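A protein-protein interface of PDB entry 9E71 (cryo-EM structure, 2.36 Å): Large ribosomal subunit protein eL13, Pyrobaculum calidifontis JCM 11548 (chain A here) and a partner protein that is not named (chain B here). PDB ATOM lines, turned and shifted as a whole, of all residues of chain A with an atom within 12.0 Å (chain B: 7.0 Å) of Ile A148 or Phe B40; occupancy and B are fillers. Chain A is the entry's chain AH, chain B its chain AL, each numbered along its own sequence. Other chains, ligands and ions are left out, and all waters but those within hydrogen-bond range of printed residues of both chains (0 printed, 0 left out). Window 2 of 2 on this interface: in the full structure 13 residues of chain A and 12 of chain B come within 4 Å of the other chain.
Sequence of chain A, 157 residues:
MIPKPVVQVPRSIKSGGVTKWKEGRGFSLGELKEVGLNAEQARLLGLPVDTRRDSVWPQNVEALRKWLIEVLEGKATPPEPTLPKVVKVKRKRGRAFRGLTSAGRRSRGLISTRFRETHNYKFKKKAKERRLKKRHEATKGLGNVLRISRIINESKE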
ATOM      1  N   LYS A 140      28.278  10.537   9.667  1.00  0.00           N
ATOM      2  CA  LYS A 140      28.037   9.368  10.499  1.00  0.00           C
ATOM      3  C   LYS A 140      27.089   9.724  11.632  1.00  0.00           C
ATOM      4  O   LYS A 140      27.215  10.780  12.254  1.00  0.00           O
ATOM      5  CB  LYS A 140      29.346   8.824  11.066  1.00  0.00           C
ATOM      6  CG  LYS A 140      30.475   8.754  10.063  1.00  0.00           C
ATOM      7  CD  LYS A 140      30.278   7.615   9.089  1.00  0.00           C
ATOM      8  CE  LYS A 140      31.343   7.630   8.002  1.00  0.00           C
ATOM      9  NZ  LYS A 140      30.945   6.840   6.813  1.00  0.00           N
ATOM     10  N   GLY A 141      26.140   8.833  11.904  1.00  0.00           N
ATOM     11  CA  GLY A 141      25.135   9.116  12.908  1.00  0.00           C
ATOM     12  C   GLY A 141      24.079  10.098  12.468  1.00  0.00           C
ATOM     13  O   GLY A 141      23.465  10.754  13.316  1.00  0.00           O
ATOM     14  N   LEU A 142      23.863  10.221  11.155  1.00  0.00           N
ATOM     15  CA  LEU A 142      22.912  11.186  10.617  1.00  0.00           C
ATOM     16  C   LEU A 142      21.498  10.912  11.107  1.00  0.00           C
ATOM     17  O   LEU A 142      20.766  11.843  11.458  1.00  0.00           O
ATOM     18  CB  LEU A 142      22.964  11.149   9.092  1.00  0.00           C
ATOM     19  CG  LEU A 142      22.000  12.049   8.326  1.00  0.00           C
ATOM     20  CD1 LEU A 142      22.409  13.493   8.476  1.00  0.00           C
ATOM     21  CD2 LEU A 142      21.943  11.654   6.860  1.00  0.00           C
ATOM     22  N   GLY A 143      21.107   9.639  11.155  1.00  0.00           N
ATOM     23  CA  GLY A 143      19.775   9.298  11.625  1.00  0.00           C
ATOM     24  C   GLY A 143      19.553   9.645  13.084  1.00  0.00           C
ATOM     25  O   GLY A 143      18.505  10.175  13.450  1.00  0.00           O
ATOM     26  N   ASN A 144      20.536   9.356  13.937  1.00  0.00           N
ATOM     27  CA  ASN A 144      20.383   9.662  15.356  1.00  0.00           C
ATOM     28  C   ASN A 144      20.397  11.162  15.605  1.00  0.00           C
ATOM     29  O   ASN A 144      19.665  11.659  16.473  1.00  0.00           O
ATOM     30  CB  ASN A 144      21.480   8.982  16.167  1.00  0.00           C
ATOM     31  CG  ASN A 144      21.004   8.553  17.527  1.00  0.00           C
ATOM     32  OD1 ASN A 144      19.813   8.374  17.748  1.00  0.00           O
ATOM     33  ND2 ASN A 144      21.930   8.402  18.454  1.00  0.00           N
ATOM     34  N   VAL A 145      21.229  11.896  14.862  1.00  0.00           N
ATOM     35  CA  VAL A 145      21.242  13.350  14.973  1.00  0.00           C
ATOM     36  C   VAL A 145      19.889  13.916  14.570  1.00  0.00           C
ATOM     37  O   VAL A 145      19.337  14.793  15.248  1.00  0.00           O
ATOM     38  CB  VAL A 145      22.380  13.943  14.122  1.00  0.00           C
ATOM     39  CG1 VAL A 145      22.244  15.444  14.031  1.00  0.00           C
ATOM     40  CG2 VAL A 145      23.725  13.567  14.702  1.00  0.00           C
ATOM     41  N   LEU A 146      19.319  13.393  13.481  1.00  0.00           N
ATOM     42  CA  LEU A 146      17.996  13.821  13.042  1.00  0.00           C
ATOM     43  C   LEU A 146      16.930  13.498  14.078  1.00  0.00           C
ATOM     44  O   LEU A 146      16.037  14.311  14.326  1.00  0.00           O
ATOM     45  CB  LEU A 146      17.642  13.156  11.715  1.00  0.00           C
ATOM     46  CG  LEU A 146      18.215  13.719  10.419  1.00  0.00           C
ATOM     47  CD1 LEU A 146      17.990  12.730   9.300  1.00  0.00           C
ATOM     48  CD2 LEU A 146      17.576  15.052  10.092  1.00  0.00           C
ATOM     49  N   ARG A 147      17.003  12.311  14.682  1.00  0.00           N
ATOM     50  CA  ARG A 147      16.004  11.898  15.661  1.00  0.00           C
ATOM     51  C   ARG A 147      16.022  12.802  16.885  1.00  0.00           C
ATOM     52  O   ARG A 147      14.974  13.287  17.333  1.00  0.00           O
ATOM     53  CB  ARG A 147      16.244  10.445  16.065  1.00  0.00           C
ATOM     54  CG  ARG A 147      15.171   9.880  16.960  1.00  0.00           C
ATOM     55  CD  ARG A 147      15.498   8.478  17.426  1.00  0.00           C
ATOM     56  NE  ARG A 147      16.740   8.422  18.181  1.00  0.00           N
ATOM     57  CZ  ARG A 147      16.810   8.321  19.499  1.00  0.00           C
ATOM     58  NH1 ARG A 147      15.722   8.296  20.247  1.00  0.00           N
ATOM     59  NH2 ARG A 147      18.000   8.239  20.081  1.00  0.00           N
ATOM     60  N   ILE A 148      17.214  13.064  17.423  1.00  0.00           N
ATOM     61  CA  ILE A 148      17.322  13.913  18.605  1.00  0.00           C
ATOM     62  C   ILE A 148      16.908  15.341  18.278  1.00  0.00           C
ATOM     63  O   ILE A 148      16.227  16.001  19.074  1.00  0.00           O
ATOM     64  CB  ILE A 148      18.748  13.856  19.176  1.00  0.00           C
ATOM     65  CG1 ILE A 148      19.109  12.423  19.565  1.00  0.00           C
ATOM     66  CG2 ILE A 148      18.873  14.779  20.361  1.00  0.00           C
ATOM     67  CD1 ILE A 148      18.419  11.936  20.805  1.00  0.00           C
ATOM     68  N   SER A 149      17.305  15.841  17.105  1.00  0.00           N
ATOM     69  CA  SER A 149      16.945  17.202  16.725  1.00  0.00           C
ATOM     70  C   SER A 149      15.445  17.342  16.515  1.00  0.00           C
ATOM     71  O   SER A 149      14.858  18.365  16.879  1.00  0.00           O
ATOM     72  CB  SER A 149      17.710  17.610  15.469  1.00  0.00           C
ATOM     73  OG  SER A 149      16.939  18.477  14.657  1.00  0.00           O
ATOM     74  N   ARG A 150      14.806  16.332  15.924  1.00  0.00           N
ATOM     75  CA  ARG A 150      13.360  16.363  15.755  1.00  0.00           C
ATOM     76  C   ARG A 150      12.649  16.348  17.097  1.00  0.00           C
ATOM     77  O   ARG A 150      11.643  17.042  17.278  1.00  0.00           O
ATOM     78  CB  ARG A 150      12.899  15.180  14.907  1.00  0.00           C
ATOM     79  CG  ARG A 150      13.216  15.296  13.435  1.00  0.00           C
ATOM     80  CD  ARG A 150      12.441  14.259  12.644  1.00  0.00           C
ATOM     81  NE  ARG A 150      12.376  12.986  13.352  1.00  0.00           N
ATOM     82  CZ  ARG A 150      13.109  11.922  13.051  1.00  0.00           C
ATOM     83  NH1 ARG A 150      13.973  11.940  12.049  1.00  0.00           N
ATOM     84  NH2 ARG A 150      12.977  10.817  13.777  1.00  0.00           N
ATOM     85  N   ILE A 151      13.153  15.554  18.047  1.00  0.00           N
ATOM     86  CA  ILE A 151      12.562  15.537  19.384  1.00  0.00           C
ATOM     87  C   ILE A 151      12.684  16.904  20.041  1.00  0.00           C
ATOM     88  O   ILE A 151      11.733  17.408  20.644  1.00  0.00           O
ATOM     89  CB  ILE A 151      13.215  14.452  20.254  1.00  0.00           C
ATOM     90  CG1 ILE A 151      12.898  13.063  19.722  1.00  0.00           C
ATOM     91  CG2 ILE A 151      12.739  14.576  21.684  1.00  0.00           C
ATOM     92  CD1 ILE A 151      13.738  11.997  20.358  1.00  0.00           C
ATOM     93  N   ILE A 152      13.856  17.527  19.929  1.00  0.00           N
ATOM     94  CA  ILE A 152      14.072  18.802  20.606  1.00  0.00           C
ATOM     95  C   ILE A 152      13.244  19.908  19.963  1.00  0.00           C
ATOM     96  O   ILE A 152      12.667  20.750  20.659  1.00  0.00           O
ATOM     97  CB  ILE A 152      15.568  19.156  20.621  1.00  0.00           C
ATOM     98  CG1 ILE A 152      16.322  18.236  21.573  1.00  0.00           C
ATOM     99  CG2 ILE A 152      15.761  20.591  21.043  1.00  0.00           C
ATOM    100  CD1 ILE A 152      17.811  18.425  21.535  1.00  0.00           C
ATOM    101  N   ASN A 153      13.170  19.929  18.634  1.00  0.00           N
ATOM    102  CA  ASN A 153      12.505  21.021  17.936  1.00  0.00           C
ATOM    103  C   ASN A 153      11.011  20.804  17.744  1.00  0.00           C
ATOM    104  O   ASN A 153      10.323  21.739  17.323  1.00  0.00           O
ATOM    105  CB  ASN A 153      13.159  21.251  16.570  1.00  0.00           C
ATOM    106  CG  ASN A 153      14.601  21.693  16.682  1.00  0.00           C
ATOM    107  OD1 ASN A 153      14.930  22.581  17.464  1.00  0.00           O
ATOM    108  ND2 ASN A 153      15.472  21.073  15.901  1.00  0.00           N
ATOM    109  N   GLU A 154      10.487  19.613  18.022  1.00  0.00           N
ATOM    110  CA  GLU A 154       9.059  19.360  17.896  1.00  0.00           C
ATOM    111  C   GLU A 154       8.396  19.039  19.227  1.00  0.00           C
ATOM    112  O   GLU A 154       7.281  18.510  19.242  1.00  0.00           O
ATOM    113  CB  GLU A 154       8.801  18.228  16.902  1.00  0.00           C
ATOM    114  CG  GLU A 154       8.862  18.648  15.445  1.00  0.00           C
ATOM    115  CD  GLU A 154      10.172  18.288  14.781  1.00  0.00           C
ATOM    116  OE1 GLU A 154      11.178  18.983  15.028  1.00  0.00           O
ATOM    117  OE2 GLU A 154      10.195  17.306  14.010  1.00  0.00           O
ATOM    118  N   SER A 155       9.050  19.341  20.341  1.00  0.00           N
ATOM    119  CA  SER A 155       8.481  19.062  21.652  1.00  0.00           C
ATOM    120  C   SER A 155       7.370  20.048  21.973  1.00  0.00           C
ATOM    121  O   SER A 155       7.632  21.223  22.226  1.00  0.00           O
ATOM    122  CB  SER A 155       9.561  19.120  22.727  1.00  0.00           C
ATOM    123  OG  SER A 155      10.178  20.394  22.739  1.00  0.00           O
ATOM    124  N   GLY B  36      29.220  12.389  19.999  1.00  0.00           N
ATOM    125  CA  GLY B  36      27.916  12.125  19.437  1.00  0.00           C
ATOM    126  C   GLY B  36      26.796  12.352  20.439  1.00  0.00           C
ATOM    127  O   GLY B  36      26.947  13.029  21.457  1.00  0.00           O
ATOM    128  N   MET B  37      25.645  11.763  20.123  1.00  0.00           N
ATOM    129  CA  MET B  37      24.443  11.880  20.949  1.00  0.00           C
ATOM    130  C   MET B  37      24.543  10.885  22.099  1.00  0.00           C
ATOM    131  O   MET B  37      23.999   9.782  22.062  1.00  0.00           O
ATOM    132  CB  MET B  37      23.195  11.634  20.111  1.00  0.00           C
ATOM    133  CG  MET B  37      23.247  12.181  18.690  1.00  0.00           C
ATOM    134  SD  MET B  37      23.019  13.965  18.582  1.00  0.00           S
ATOM    135  CE  MET B  37      24.649  14.567  18.980  1.00  0.00           C
ATOM    136  N   VAL B  38      25.257  11.289  23.145  1.00  0.00           N
ATOM    137  CA  VAL B  38      25.481  10.434  24.300  1.00  0.00           C
ATOM    138  C   VAL B  38      25.216  11.217  25.576  1.00  0.00           C
ATOM    139  O   VAL B  38      25.158  12.448  25.583  1.00  0.00           O
ATOM    140  CB  VAL B  38      26.906   9.845  24.325  1.00  0.00           C
ATOM    141  CG1 VAL B  38      27.150   9.019  23.082  1.00  0.00           C
ATOM    142  CG2 VAL B  38      27.935  10.946  24.460  1.00  0.00           C
ATOM    143  N   GLY B  39      25.058  10.474  26.666  1.00  0.00           N
ATOM    144  CA  GLY B  39      24.864  11.040  27.981  1.00  0.00           C
ATOM    145  C   GLY B  39      23.439  11.376  28.341  1.00  0.00           C
ATOM    146  O   GLY B  39      23.207  11.913  29.428  1.00  0.00           O
ATOM    147  N   PHE B  40      22.473  11.053  27.483  1.00  0.00           N
ATOM    148  CA  PHE B  40      21.102  11.502  27.680  1.00  0.00           C
ATOM    149  C   PHE B  40      20.381  10.776  28.800  1.00  0.00           C
ATOM    150  O   PHE B  40      19.279  11.187  29.160  1.00  0.00           O
ATOM    151  CB  PHE B  40      20.312  11.352  26.385  1.00  0.00           C
ATOM    152  CG  PHE B  40      20.627  12.397  25.374  1.00  0.00           C
ATOM    153  CD1 PHE B  40      20.369  13.726  25.639  1.00  0.00           C
ATOM    154  CD2 PHE B  40      21.193  12.059  24.167  1.00  0.00           C
ATOM    155  CE1 PHE B  40      20.665  14.692  24.719  1.00  0.00           C
ATOM    156  CE2 PHE B  40      21.490  13.025  23.243  1.00  0.00           C
ATOM    157  CZ  PHE B  40      21.225  14.342  23.519  1.00  0.00           C
ATOM    158  N   HIS B  41      20.954   9.713  29.349  1.00  0.00           N
ATOM    159  CA  HIS B  41      20.382   9.064  30.514  1.00  0.00           C
ATOM    160  C   HIS B  41      21.202   9.266  31.774  1.00  0.00           C
ATOM    161  O   HIS B  41      20.778   8.820  32.841  1.00  0.00           O
ATOM    162  CB  HIS B  41      20.193   7.567  30.263  1.00  0.00           C
ATOM    163  CG  HIS B  41      18.893   7.040  30.778  1.00  0.00           C
ATOM    164  ND1 HIS B  41      18.609   6.952  32.123  1.00  0.00           N
ATOM    165  CD2 HIS B  41      17.788   6.601  30.132  1.00  0.00           C
ATOM    166  CE1 HIS B  41      17.390   6.477  32.283  1.00  0.00           C
ATOM    167  NE2 HIS B  41      16.872   6.250  31.091  1.00  0.00           N
ATOM    168  N   LYS B  42      22.367   9.903  31.691  1.00  0.00           N
ATOM    169  CA  LYS B  42      23.172  10.131  32.884  1.00  0.00           C
ATOM    170  C   LYS B  42      23.351  11.607  33.209  1.00  0.00           C
ATOM    171  O   LYS B  42      22.912  12.045  34.273  1.00  0.00           O
ATOM    172  CB  LYS B  42      24.528   9.439  32.730  1.00  0.00           C
ATOM    173  CG  LYS B  42      24.430   7.935  32.703  1.00  0.00           C
ATOM    174  CD  LYS B  42      23.869   7.394  34.004  1.00  0.00           C
ATOM    175  CE  LYS B  42      24.701   7.834  35.177  1.00  0.00           C
ATOM    176  NZ  LYS B  42      24.406   7.053  36.401  1.00  0.00           N
ATOM    177  N   HIS B  43      23.948  12.400  32.327  1.00  0.00           N
ATOM    178  CA  HIS B  43      24.204  13.796  32.640  1.00  0.00           C
ATOM    179  C   HIS B  43      23.480  14.750  31.705  1.00  0.00           C
ATOM    180  O   HIS B  43      23.597  15.964  31.870  1.00  0.00           O
ATOM    181  CB  HIS B  43      25.714  14.091  32.649  1.00  0.00           C
ATOM    182  CG  HIS B  43      26.431  13.685  31.400  1.00  0.00           C
ATOM    183  ND1 HIS B  43      26.708  12.373  31.091  1.00  0.00           N
ATOM    184  CD2 HIS B  43      26.952  14.425  30.396  1.00  0.00           C
ATOM    185  CE1 HIS B  43      27.347  12.321  29.937  1.00  0.00           C
ATOM    186  NE2 HIS B  43      27.513  13.553  29.497  1.00  0.00           N
ATOM    187  N   LYS B  44      22.729  14.233  30.738  1.00  0.00           N
ATOM    188  CA  LYS B  44      21.803  15.030  29.948  1.00  0.00           C
ATOM    189  C   LYS B  44      20.365  14.588  30.168  1.00  0.00           C
ATOM    190  O   LYS B  44      19.466  14.937  29.387  1.00  0.00           O
ATOM    191  CB  LYS B  44      22.201  14.970  28.478  1.00  0.00           C
ATOM    192  CG  LYS B  44      23.623  15.447  28.267  1.00  0.00           C
ATOM    193  CD  LYS B  44      24.009  15.484  26.817  1.00  0.00           C
ATOM    194  CE  LYS B  44      25.479  15.811  26.669  1.00  0.00           C
ATOM    195  NZ  LYS B  44      25.980  15.516  25.312  1.00  0.00           N
ATOM    196  N   TRP B  45      20.131  13.842  31.250  1.00  0.00           N
ATOM    197  CA  TRP B  45      18.784  13.481  31.661  1.00  0.00           C
ATOM    198  C   TRP B  45      17.953  14.706  31.992  1.00  0.00           C
ATOM    199  O   TRP B  45      16.732  14.674  31.849  1.00  0.00           O
ATOM    200  CB  TRP B  45      18.854  12.552  32.865  1.00  0.00           C
ATOM    201  CG  TRP B  45      17.583  11.861  33.214  1.00  0.00           C
ATOM    202  CD1 TRP B  45      16.914  11.937  34.388  1.00  0.00           C
ATOM    203  CD2 TRP B  45      16.846  10.957  32.389  1.00  0.00           C
ATOM    204  NE1 TRP B  45      15.800  11.142  34.351  1.00  0.00           N
ATOM    205  CE2 TRP B  45      15.738  10.526  33.132  1.00  0.00           C
ATOM    206  CE3 TRP B  45      17.017  10.471  31.093  1.00  0.00           C
ATOM    207  CZ2 TRP B  45      14.811   9.625  32.625  1.00  0.00           C
ATOM    208  CZ3 TRP B  45      16.091   9.592  30.589  1.00  0.00           C
ATOM    209  CH2 TRP B  45      14.998   9.183  31.349  1.00  0.00           C
ATOM    210  N   SER B  46      18.587  15.785  32.451  1.00  0.00           N
ATOM    211  CA  SER B  46      17.866  17.038  32.627  1.00  0.00           C
ATOM    212  C   SER B  46      17.348  17.564  31.293  1.00  0.00           C
ATOM    213  O   SER B  46      16.236  18.092  31.218  1.00  0.00           O
ATOM    214  CB  SER B  46      18.766  18.059  33.315  1.00  0.00           C
ATOM    215  OG  SER B  46      20.127  17.743  33.117  1.00  0.00           O
ATOM    216  N   LEU B  47      18.130  17.408  30.228  1.00  0.00           N
ATOM    217  CA  LEU B  47      17.652  17.750  28.895  1.00  0.00           C
ATOM    218  C   LEU B  47      16.479  16.865  28.492  1.00  0.00           C
ATOM    219  O   LEU B  47      15.498  17.337  27.895  1.00  0.00           O
ATOM    220  CB  LEU B  47      18.804  17.622  27.901  1.00  0.00           C
ATOM    221  CG  LEU B  47      18.801  18.485  26.647  1.00  0.00           C
ATOM    222  CD1 LEU B  47      17.800  17.965  25.649  1.00  0.00           C
ATOM    223  CD2 LEU B  47      18.495  19.918  27.007  1.00  0.00           C
ATOM    224  N   VAL B  48      16.561  15.575  28.825  1.00  0.00           N
ATOM    225  CA  VAL B  48      15.474  14.652  28.505  1.00  0.00           C
ATOM    226  C   VAL B  48      14.203  15.016  29.264  1.00  0.00           C
ATOM    227  O   VAL B  48      13.100  14.925  28.726  1.00  0.00           O
ATOM    228  CB  VAL B  48      15.900  13.203  28.790  1.00  0.00           C
ATOM    229  CG1 VAL B  48      14.681  12.312  28.854  1.00  0.00           C
ATOM    230  CG2 VAL B  48      16.860  12.726  27.724  1.00  0.00           C
ATOM    231  N   MET B  49      14.332  15.412  30.528  1.00  0.00           N
ATOM    232  CA  MET B  49      13.173  15.859  31.299  1.00  0.00           C
ATOM    233  C   MET B  49      12.641  17.203  30.837  1.00  0.00           C
ATOM    234  O   MET B  49      11.447  17.472  30.991  1.00  0.00           O
ATOM    235  CB  MET B  49      13.510  15.895  32.787  1.00  0.00           C
ATOM    236  CG  MET B  49      13.603  14.530  33.385  1.00  0.00           C
ATOM    237  SD  MET B  49      12.090  13.723  32.839  1.00  0.00           S
ATOM    238  CE  MET B  49      12.631  12.087  32.503  1.00  0.00           C
ATOM    239  N   PRO B  59      10.340   9.852  23.950  1.00  0.00           N
ATOM    240  CA  PRO B  59      10.859   9.995  22.576  1.00  0.00           C
ATOM    241  C   PRO B  59      12.358   9.780  22.484  1.00  0.00           C
ATOM    242  O   PRO B  59      12.856   9.319  21.453  1.00  0.00           O
ATOM    243  CB  PRO B  59      10.442  11.414  22.167  1.00  0.00           C
ATOM    244  CG  PRO B  59       9.839  12.040  23.333  1.00  0.00           C
ATOM    245  CD  PRO B  59       9.777  11.103  24.483  1.00  0.00           C
ATOM    246  N   PHE B  60      13.082  10.044  23.569  1.00  0.00           N
ATOM    247  CA  PHE B  60      14.503   9.741  23.592  1.00  0.00           C
ATOM    248  C   PHE B  60      14.750   8.245  23.736  1.00  0.00           C
ATOM    249  O   PHE B  60      15.621   7.689  23.059  1.00  0.00           O
ATOM    250  CB  PHE B  60      15.178  10.511  24.725  1.00  0.00           C
ATOM    251  CG  PHE B  60      15.168  11.997  24.533  1.00  0.00           C
ATOM    252  CD1 PHE B  60      14.099  12.757  24.967  1.00  0.00           C
ATOM    253  CD2 PHE B  60      16.229  12.635  23.918  1.00  0.00           C
ATOM    254  CE1 PHE B  60      14.088  14.120  24.791  1.00  0.00           C
ATOM    255  CE2 PHE B  60      16.222  14.001  23.741  1.00  0.00           C
ATOM    256  CZ  PHE B  60      15.149  14.743  24.179  1.00  0.00           C
ATOM    257  N   TYR B  61      13.988   7.572  24.599  1.00  0.00           N
ATOM    258  CA  TYR B  61      14.234   6.178  24.937  1.00  0.00           C
ATOM    259  C   TYR B  61      12.933   5.393  24.985  1.00  0.00           C
ATOM    260  O   TYR B  61      11.958   5.816  25.606  1.00  0.00           O
ATOM    261  CB  TYR B  61      14.924   6.042  26.294  1.00  0.00           C
ATOM    262  CG  TYR B  61      16.337   6.551  26.341  1.00  0.00           C
ATOM    263  CD1 TYR B  61      17.363   5.843  25.748  1.00  0.00           C
ATOM    264  CD2 TYR B  61      16.647   7.731  26.997  1.00  0.00           C
ATOM    265  CE1 TYR B  61      18.654   6.297  25.794  1.00  0.00           C
ATOM    266  CE2 TYR B  61      17.939   8.195  27.049  1.00  0.00           C
ATOM    267  CZ  TYR B  61      18.939   7.473  26.445  1.00  0.00           C
ATOM    268  OH  TYR B  61      20.233   7.921  26.488  1.00  0.00           O
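Of the 16 printed residues of chain A, 5 touch a printed residue of chain B. Hydrophobic or aromatic side chains of chain A within 4 Å of the printed part of chain B: Val A145, Ile A148 and Ile A151. Printed residues of chain B that touch a printed residue of chain A: Met B37, Phe B40, Pro B59 and Phe B60. Hydrophobic or aromatic side chains of chain B that line the printed part of chain A: Met B37, Phe B40, Pro B59 and Phe B60. Among the printed residues, no Asp or Glu carboxylate lies within 4 Å of a Lys or Arg side-chain nitrogen of the other chain.
The backbone carbonyl oxygen of Pro B59 is in hydrogen-bond range of the guanidinium group of Arg A147 (3.3 Å). The backbone carbonyl oxygen (O) of Phe B60 is in hydrogen-bond range of the guanidinium group (NH1) of Arg A147.
Among the printed residues, pairs that only touch across the chains: Ile A151 with Pro B59 (3.0 Å), Ile A151 with Phe B60 (3.4 Å), Asn A144 with Met B37 (3.8 Å), Ile A148 with Phe B60 (3.9 Å), Ile A148 with Phe B40 (3.96 Å) and Val A145 with Met B37 (3.96 Å).
The side-chain amide oxygen (OD1) of Asn A144 lies within hydrogen-bond range of the guanidinium group (NH2) of Arg A147 (3.0 Å). N of Trp B45 sits close to O of Phe B40, at 3.5 Å.
Of chain A, only Ile A148 comes within 4 Å of Phe B40. Of chain A, only Asn A144 and Val A145 come within 4 Å of Met B37. No residue of chain A comes within 4 Å of Val B38. No residue of chain A comes within 4 Å of Gly B39. No residue of chain A comes within 4 Å of Lys B44. No residue of chain A comes within 4 Å of Trp B45. No residue of chain A comes within 4 Å of Leu B47. No residue of chain A comes within 4 Å of Val B48. Phe B60 touches just these residues of chain A: Arg A147, Ile A148 and Ile A151. Printed residues of chain B within 4 Å of Ile A151: Pro B59 (3.0 Å) and Phe B60 (3.4 Å). Printed residues of chain B within 4 Å of Arg A147: Pro B59 and Phe B60. Printed residues of chain B within 4 Å of Asn A144: Met B37. Of the printed residues of chain B, Val A145 touches Met B37. Lys A140 touches none of the printed residues of chain B. Lys B42 touches none of the printed residues of chain A. The nearest residue of chain B that does not touch Ile A148 is Met B37 (4.2 Å). The nearest residue of chain A that does not touch Phe B40 is Ile A152 (5.7 Å).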
